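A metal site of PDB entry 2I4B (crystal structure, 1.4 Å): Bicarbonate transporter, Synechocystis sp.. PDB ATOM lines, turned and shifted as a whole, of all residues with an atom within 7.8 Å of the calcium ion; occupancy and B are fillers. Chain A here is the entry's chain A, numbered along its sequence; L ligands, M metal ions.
The backbone carbonyl oxygen (O) of Asn 129 sits at hydrogen-bond distance from the backbone NH (N) of Thr 238, 3.0 Å away. The indole nitrogen (NE1) of Trp 178 lies within hydrogen-bond range of the side-chain carboxylate (OE1) of Glu 247, 3.0 Å away. N of Gln 175 lies close to NE2 of Gln 98 (3.1 Å). The side-chain amide nitrogen (ND2) of Asn 129 sits at hydrogen-bond distance from the backbone carbonyl oxygen (O) of Gln 127 (3.0 Å). The side-chain carboxylate (OE1) of Glu 247 lies within hydrogen-bond range of a ring nitrogen (NE2) of His 245. The side-chain amide nitrogen of Asn 174 is in hydrogen-bond range of the backbone carbonyl oxygen of Glu 247 (3.0 Å). The side-chain carboxylate (OE1) of Glu 248 lies within hydrogen-bond range of the side-chain amide nitrogen (NE2) of Gln 96 (2.6 Å). The backbone carbonyl oxygen (O) of Gln 175 sits at hydrogen-bond distance from the side-chain hydroxyl (OG) of Ser 217 (2.7 Å).
Within 4 Å of the calcium ion: Glu 47, Asn 129, Gln 175, Glu 247 and Glu 248.
The calcium ion is bound by OE2 of Glu 47 (2.3 Å). OE2 of Glu 247 binds the calcium ion, 2.3 Å away. OE1 of Gln 175 is bound to the calcium ion, 2.4 Å away. O1 of the ligand binds the calcium ion, at 2.4 Å. The calcium ion is bound by the side-chain amide oxygen (OD1) of Asn 129 (2.5 Å). The calcium ion is bound by the side-chain carboxylate (OE2) of Glu 248 (2.6 Å). The calcium ion has six donor atoms within binding distance.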
ATOM      1  N   ILE A  45      27.312  26.195 -20.177  1.00  0.00           N
ATOM      2  CA  ILE A  45      27.072  24.778 -20.387  1.00  0.00           C
ATOM      3  C   ILE A  45      28.446  24.088 -20.449  1.00  0.00           C
ATOM      4  O   ILE A  45      29.462  24.756 -20.661  1.00  0.00           O
ATOM      5  CB  ILE A  45      26.291  24.528 -21.692  1.00  0.00           C
ATOM      6  CG1 ILE A  45      26.926  25.303 -22.847  1.00  0.00           C
ATOM      7  CG2 ILE A  45      24.830  24.940 -21.491  1.00  0.00           C
ATOM      8  CD1 ILE A  45      26.231  25.126 -24.172  1.00  0.00           C
ATOM      9  N   VAL A  46      28.483  22.768 -20.275  1.00  0.00           N
ATOM     10  CA  VAL A  46      29.765  22.058 -20.237  1.00  0.00           C
ATOM     11  C   VAL A  46      30.702  22.283 -21.421  1.00  0.00           C
ATOM     12  O   VAL A  46      31.913  22.110 -21.295  1.00  0.00           O
ATOM     13  CB  VAL A  46      29.561  20.532 -20.035  1.00  0.00           C
ATOM     14  CG1 VAL A  46      28.876  20.279 -18.694  1.00  0.00           C
ATOM     15  CG2 VAL A  46      28.754  19.944 -21.183  1.00  0.00           C
ATOM     16  N   GLU A  47      30.146  22.677 -22.566  1.00  0.00           N
ATOM     17  CA  GLU A  47      30.954  22.948 -23.746  1.00  0.00           C
ATOM     18  C   GLU A  47      31.971  24.072 -23.493  1.00  0.00           C
ATOM     19  O   GLU A  47      32.993  24.161 -24.177  1.00  0.00           O
ATOM     20  CB  GLU A  47      30.050  23.348 -24.925  1.00  0.00           C
ATOM     21  CG  GLU A  47      29.156  22.210 -25.476  1.00  0.00           C
ATOM     22  CD  GLU A  47      27.811  22.079 -24.787  1.00  0.00           C
ATOM     23  OE1 GLU A  47      27.732  22.270 -23.554  1.00  0.00           O
ATOM     24  OE2 GLU A  47      26.826  21.770 -25.495  1.00  0.00           O
ATOM     25  N   TRP A  76      22.420  32.792 -27.205  1.00  0.00           N
ATOM     26  CA  TRP A  76      23.096  32.683 -28.480  1.00  0.00           C
ATOM     27  C   TRP A  76      22.919  33.879 -29.405  1.00  0.00           C
ATOM     28  O   TRP A  76      23.851  34.239 -30.146  1.00  0.00           O
ATOM     29  CB  TRP A  76      22.700  31.367 -29.168  1.00  0.00           C
ATOM     30  CG  TRP A  76      23.369  30.172 -28.519  1.00  0.00           C
ATOM     31  CD1 TRP A  76      22.767  29.167 -27.816  1.00  0.00           C
ATOM     32  CD2 TRP A  76      24.777  29.903 -28.481  1.00  0.00           C
ATOM     33  NE1 TRP A  76      23.717  28.289 -27.333  1.00  0.00           N
ATOM     34  CE2 TRP A  76      24.965  28.725 -27.732  1.00  0.00           C
ATOM     35  CE3 TRP A  76      25.901  30.550 -29.010  1.00  0.00           C
ATOM     36  CZ2 TRP A  76      26.226  28.170 -27.503  1.00  0.00           C
ATOM     37  CZ3 TRP A  76      27.163  30.005 -28.779  1.00  0.00           C
ATOM     38  CH2 TRP A  76      27.310  28.823 -28.032  1.00  0.00           C
ATOM     39  N   GLN A  96      33.000  30.573 -27.841  1.00  0.00           N
ATOM     40  CA  GLN A  96      32.364  29.258 -27.978  1.00  0.00           C
ATOM     41  C   GLN A  96      31.181  29.404 -28.922  1.00  0.00           C
ATOM     42  O   GLN A  96      30.414  30.357 -28.805  1.00  0.00           O
ATOM     43  CB  GLN A  96      31.888  28.823 -26.595  1.00  0.00           C
ATOM     44  CG  GLN A  96      30.955  27.633 -26.514  1.00  0.00           C
ATOM     45  CD  GLN A  96      30.228  27.610 -25.184  1.00  0.00           C
ATOM     46  OE1 GLN A  96      30.644  28.277 -24.237  1.00  0.00           O
ATOM     47  NE2 GLN A  96      29.131  26.854 -25.101  1.00  0.00           N
ATOM     48  N   TRP A  97      31.023  28.448 -29.842  1.00  0.00           N
ATOM     49  CA  TRP A  97      29.921  28.515 -30.804  1.00  0.00           C
ATOM     50  C   TRP A  97      29.304  27.195 -31.205  1.00  0.00           C
ATOM     51  O   TRP A  97      29.970  26.164 -31.237  1.00  0.00           O
ATOM     52  CB  TRP A  97      30.381  29.146 -32.116  1.00  0.00           C
ATOM     53  CG  TRP A  97      31.043  30.435 -31.946  1.00  0.00           C
ATOM     54  CD1 TRP A  97      32.382  30.669 -31.886  1.00  0.00           C
ATOM     55  CD2 TRP A  97      30.399  31.698 -31.743  1.00  0.00           C
ATOM     56  NE1 TRP A  97      32.619  32.003 -31.656  1.00  0.00           N
ATOM     57  CE2 TRP A  97      31.424  32.657 -31.566  1.00  0.00           C
ATOM     58  CE3 TRP A  97      29.065  32.101 -31.697  1.00  0.00           C
ATOM     59  CZ2 TRP A  97      31.137  34.005 -31.329  1.00  0.00           C
ATOM     60  CZ3 TRP A  97      28.777  33.438 -31.462  1.00  0.00           C
ATOM     61  CH2 TRP A  97      29.809  34.377 -31.289  1.00  0.00           C
ATOM     62  N   GLN A  98      28.008  27.245 -31.505  1.00  0.00           N
ATOM     63  CA  GLN A  98      27.339  26.090 -32.059  1.00  0.00           C
ATOM     64  C   GLN A  98      27.654  26.223 -33.560  1.00  0.00           C
ATOM     65  O   GLN A  98      27.847  27.328 -34.064  1.00  0.00           O
ATOM     66  CB  GLN A  98      25.838  26.182 -31.852  1.00  0.00           C
ATOM     67  CG  GLN A  98      25.388  25.822 -30.434  1.00  0.00           C
ATOM     68  CD  GLN A  98      23.885  25.792 -30.315  1.00  0.00           C
ATOM     69  OE1 GLN A  98      23.250  26.769 -29.915  1.00  0.00           O
ATOM     70  NE2 GLN A  98      23.289  24.661 -30.705  1.00  0.00           N
ATOM     71  N   ILE A 125      34.616  20.218 -27.529  1.00  0.00           N
ATOM     72  CA  ILE A 125      34.119  19.050 -26.841  1.00  0.00           C
ATOM     73  C   ILE A 125      33.267  18.200 -27.766  1.00  0.00           C
ATOM     74  O   ILE A 125      32.940  18.623 -28.876  1.00  0.00           O
ATOM     75  CB  ILE A 125      33.181  19.538 -25.694  1.00  0.00           C
ATOM     76  CG1 ILE A 125      32.672  18.402 -24.812  1.00  0.00           C
ATOM     77  CG2 ILE A 125      32.011  20.297 -26.319  1.00  0.00           C
ATOM     78  CD1 ILE A 125      31.711  18.858 -23.706  1.00  0.00           C
ATOM     79  N   GLN A 127      29.844  15.357 -27.273  1.00  0.00           N
ATOM     80  CA  GLN A 127      28.840  14.844 -26.340  1.00  0.00           C
ATOM     81  C   GLN A 127      28.447  15.838 -25.238  1.00  0.00           C
ATOM     82  O   GLN A 127      28.638  17.048 -25.407  1.00  0.00           O
ATOM     83  CB  GLN A 127      29.311  13.482 -25.804  1.00  0.00           C
ATOM     84  CG  GLN A 127      29.714  12.586 -26.988  1.00  0.00           C
ATOM     85  CD  GLN A 127      30.116  11.171 -26.630  1.00  0.00           C
ATOM     86  OE1 GLN A 127      30.657  10.908 -25.557  1.00  0.00           O
ATOM     87  NE2 GLN A 127      29.870  10.256 -27.546  1.00  0.00           N
ATOM     88  N   GLY A 128      27.887  15.353 -24.143  1.00  0.00           N
ATOM     89  CA  GLY A 128      27.455  16.244 -23.076  1.00  0.00           C
ATOM     90  C   GLY A 128      26.123  16.913 -23.429  1.00  0.00           C
ATOM     91  O   GLY A 128      25.721  17.897 -22.791  1.00  0.00           O
ATOM     92  N   ASN A 129      25.448  16.395 -24.443  1.00  0.00           N
ATOM     93  CA  ASN A 129      24.160  16.934 -24.865  1.00  0.00           C
ATOM     94  C   ASN A 129      23.106  15.820 -24.890  1.00  0.00           C
ATOM     95  O   ASN A 129      23.450  14.641 -24.869  1.00  0.00           O
ATOM     96  CB  ASN A 129      24.283  17.575 -26.253  1.00  0.00           C
ATOM     97  CG  ASN A 129      25.030  18.908 -26.221  1.00  0.00           C
ATOM     98  OD1 ASN A 129      24.424  19.956 -26.418  1.00  0.00           O
ATOM     99  ND2 ASN A 129      26.335  18.862 -25.974  1.00  0.00           N
ATOM    100  N   GLY A 130      21.826  16.203 -24.911  1.00  0.00           N
ATOM    101  CA  GLY A 130      20.775  15.199 -24.923  1.00  0.00           C
ATOM    102  C   GLY A 130      19.392  15.791 -25.161  1.00  0.00           C
ATOM    103  O   GLY A 130      19.228  17.008 -25.176  1.00  0.00           O
ATOM    104  N   THR A 169      17.907  25.879 -28.703  1.00  0.00           N
ATOM    105  CA  THR A 169      18.402  27.136 -28.138  1.00  0.00           C
ATOM    106  C   THR A 169      18.747  28.217 -29.166  1.00  0.00           C
ATOM    107  O   THR A 169      19.027  29.359 -28.806  1.00  0.00           O
ATOM    108  CB  THR A 169      19.643  26.887 -27.253  1.00  0.00           C
ATOM    109  OG1 THR A 169      19.381  25.810 -26.357  1.00  0.00           O
ATOM    110  CG2 THR A 169      19.968  28.128 -26.444  1.00  0.00           C
ATOM    111  N   ASN A 174      23.647  23.272 -34.035  1.00  0.00           N
ATOM    112  CA  ASN A 174      23.684  22.038 -33.249  1.00  0.00           C
ATOM    113  C   ASN A 174      22.409  21.462 -32.646  1.00  0.00           C
ATOM    114  O   ASN A 174      21.901  20.464 -33.152  1.00  0.00           O
ATOM    115  CB  ASN A 174      24.712  22.175 -32.119  1.00  0.00           C
ATOM    116  CG  ASN A 174      26.127  22.157 -32.627  1.00  0.00           C
ATOM    117  OD1 ASN A 174      26.460  22.874 -33.557  1.00  0.00           O
ATOM    118  ND2 ASN A 174      26.969  21.349 -32.017  1.00  0.00           N
ATOM    119  N   GLN A 175      21.895  22.070 -31.589  1.00  0.00           N
ATOM    120  CA  GLN A 175      20.714  21.546 -30.917  1.00  0.00           C
ATOM    121  C   GLN A 175      19.504  21.358 -31.837  1.00  0.00           C
ATOM    122  O   GLN A 175      18.746  20.401 -31.682  1.00  0.00           O
ATOM    123  CB  GLN A 175      20.330  22.428 -29.728  1.00  0.00           C
ATOM    124  CG  GLN A 175      21.520  22.846 -28.855  1.00  0.00           C
ATOM    125  CD  GLN A 175      22.464  21.693 -28.542  1.00  0.00           C
ATOM    126  OE1 GLN A 175      23.659  21.787 -28.810  1.00  0.00           O
ATOM    127  NE2 GLN A 175      21.930  20.612 -27.957  1.00  0.00           N
ATOM    128  N   TRP A 178      20.303  18.237 -33.785  1.00  0.00           N
ATOM    129  CA  TRP A 178      20.179  17.005 -33.024  1.00  0.00           C
ATOM    130  C   TRP A 178      18.730  16.568 -32.859  1.00  0.00           C
ATOM    131  O   TRP A 178      18.393  15.410 -33.105  1.00  0.00           O
ATOM    132  CB  TRP A 178      20.830  17.132 -31.654  1.00  0.00           C
ATOM    133  CG  TRP A 178      22.276  17.562 -31.655  1.00  0.00           C
ATOM    134  CD1 TRP A 178      22.900  18.271 -30.676  1.00  0.00           C
ATOM    135  CD2 TRP A 178      23.271  17.304 -32.659  1.00  0.00           C
ATOM    136  NE1 TRP A 178      24.225  18.467 -31.001  1.00  0.00           N
ATOM    137  CE2 TRP A 178      24.478  17.887 -32.212  1.00  0.00           C
ATOM    138  CE3 TRP A 178      23.272  16.625 -33.889  1.00  0.00           C
ATOM    139  CZ2 TRP A 178      25.666  17.832 -32.964  1.00  0.00           C
ATOM    140  CZ3 TRP A 178      24.463  16.578 -34.630  1.00  0.00           C
ATOM    141  CH2 TRP A 178      25.625  17.175 -34.160  1.00  0.00           C
ATOM    142  N   SER A 217      15.756  20.057 -27.029  1.00  0.00           N
ATOM    143  CA  SER A 217      17.143  19.724 -27.315  1.00  0.00           C
ATOM    144  C   SER A 217      18.038  20.493 -26.349  1.00  0.00           C
ATOM    145  O   SER A 217      18.260  21.699 -26.515  1.00  0.00           O
ATOM    146  CB  SER A 217      17.464  20.093 -28.755  1.00  0.00           C
ATOM    147  OG  SER A 217      18.587  19.375 -29.210  1.00  0.00           O
ATOM    148  N   THR A 218      18.566  19.785 -25.364  1.00  0.00           N
ATOM    149  CA  THR A 218      19.395  20.416 -24.360  1.00  0.00           C
ATOM    150  C   THR A 218      20.745  19.739 -24.136  1.00  0.00           C
ATOM    151  O   THR A 218      21.166  18.890 -24.926  1.00  0.00           O
ATOM    152  CB  THR A 218      18.618  20.489 -23.016  1.00  0.00           C
ATOM    153  OG1 THR A 218      19.324  21.326 -22.090  1.00  0.00           O
ATOM    154  CG2 THR A 218      18.459  19.097 -22.424  1.00  0.00           C
ATOM    155  N   GLY A 219      21.414  20.128 -23.056  1.00  0.00           N
ATOM    156  CA  GLY A 219      22.715  19.569 -22.743  1.00  0.00           C
ATOM    157  C   GLY A 219      23.039  19.849 -21.289  1.00  0.00           C
ATOM    158  O   GLY A 219      22.343  20.614 -20.625  1.00  0.00           O
ATOM    159  N   ASP A 220      24.120  19.248 -20.798  1.00  0.00           N
ATOM    160  CA  ASP A 220      24.539  19.423 -19.422  1.00  0.00           C
ATOM    161  C   ASP A 220      24.880  20.862 -19.056  1.00  0.00           C
ATOM    162  O   ASP A 220      25.497  21.590 -19.841  1.00  0.00           O
ATOM    163  CB  ASP A 220      25.698  18.488 -19.118  1.00  0.00           C
ATOM    164  CG  ASP A 220      25.352  17.042 -19.411  1.00  0.00           C
ATOM    165  OD1 ASP A 220      24.171  16.672 -19.235  1.00  0.00           O
ATOM    166  OD2 ASP A 220      26.243  16.267 -19.821  1.00  0.00           O
ATOM    167  N   THR A 238      23.072  12.738 -27.099  1.00  0.00           N
ATOM    168  CA  THR A 238      23.622  12.875 -28.436  1.00  0.00           C
ATOM    169  C   THR A 238      24.743  11.832 -28.593  1.00  0.00           C
ATOM    170  O   THR A 238      25.066  11.415 -29.705  1.00  0.00           O
ATOM    171  CB  THR A 238      24.120  14.323 -28.715  1.00  0.00           C
ATOM    172  OG1 THR A 238      25.052  14.718 -27.703  1.00  0.00           O
ATOM    173  CG2 THR A 238      22.936  15.294 -28.750  1.00  0.00           C
ATOM    174  N   HIS A 245      30.279  12.661 -31.822  1.00  0.00           N
ATOM    175  CA  HIS A 245      29.889  13.648 -32.820  1.00  0.00           C
ATOM    176  C   HIS A 245      30.566  15.001 -32.614  1.00  0.00           C
ATOM    177  O   HIS A 245      30.931  15.373 -31.499  1.00  0.00           O
ATOM    178  CB  HIS A 245      28.380  13.887 -32.747  1.00  0.00           C
ATOM    179  CG  HIS A 245      27.934  14.544 -31.471  1.00  0.00           C
ATOM    180  ND1 HIS A 245      27.669  13.844 -30.306  1.00  0.00           N
ATOM    181  CD2 HIS A 245      27.742  15.853 -31.167  1.00  0.00           C
ATOM    182  CE1 HIS A 245      27.342  14.692 -29.342  1.00  0.00           C
ATOM    183  NE2 HIS A 245      27.382  15.917 -29.847  1.00  0.00           N
ATOM    184  N   GLU A 247      30.774  18.797 -31.868  1.00  0.00           N
ATOM    185  CA  GLU A 247      29.821  19.589 -31.080  1.00  0.00           C
ATOM    186  C   GLU A 247      30.092  21.095 -31.165  1.00  0.00           C
ATOM    187  O   GLU A 247      29.897  21.688 -32.220  1.00  0.00           O
ATOM    188  CB  GLU A 247      29.808  19.091 -29.635  1.00  0.00           C
ATOM    189  CG  GLU A 247      28.786  19.765 -28.702  1.00  0.00           C
ATOM    190  CD  GLU A 247      27.387  19.857 -29.273  1.00  0.00           C
ATOM    191  OE1 GLU A 247      26.972  18.968 -30.044  1.00  0.00           O
ATOM    192  OE2 GLU A 247      26.683  20.842 -28.950  1.00  0.00           O
ATOM    193  N   GLU A 248      30.537  21.714 -30.075  1.00  0.00           N
ATOM    194  CA  GLU A 248      30.785  23.155 -30.102  1.00  0.00           C
ATOM    195  C   GLU A 248      32.250  23.475 -30.328  1.00  0.00           C
ATOM    196  O   GLU A 248      33.134  22.674 -30.016  1.00  0.00           O
ATOM    197  CB  GLU A 248      30.212  23.831 -28.847  1.00  0.00           C
ATOM    198  CG  GLU A 248      28.668  23.873 -28.885  1.00  0.00           C
ATOM    199  CD  GLU A 248      28.035  24.617 -27.731  1.00  0.00           C
ATOM    200  OE1 GLU A 248      28.527  25.693 -27.365  1.00  0.00           O
ATOM    201  OE2 GLU A 248      27.009  24.130 -27.203  1.00  0.00           O
HETATM  202  C1  LIG L   1      23.778  24.767 -26.593  1.00  0.00           C
HETATM  203  O1  LIG L   1      23.928  23.523 -26.319  1.00  0.00           O
HETATM  204  O2  LIG L   1      24.656  25.390 -27.276  1.00  0.00           O
HETATM  205  O3  LIG L   1      22.698  25.419 -26.146  1.00  0.00           O
HETATM  206 CA    CA M   1      25.543  22.024 -27.332  1.00  0.00          CA
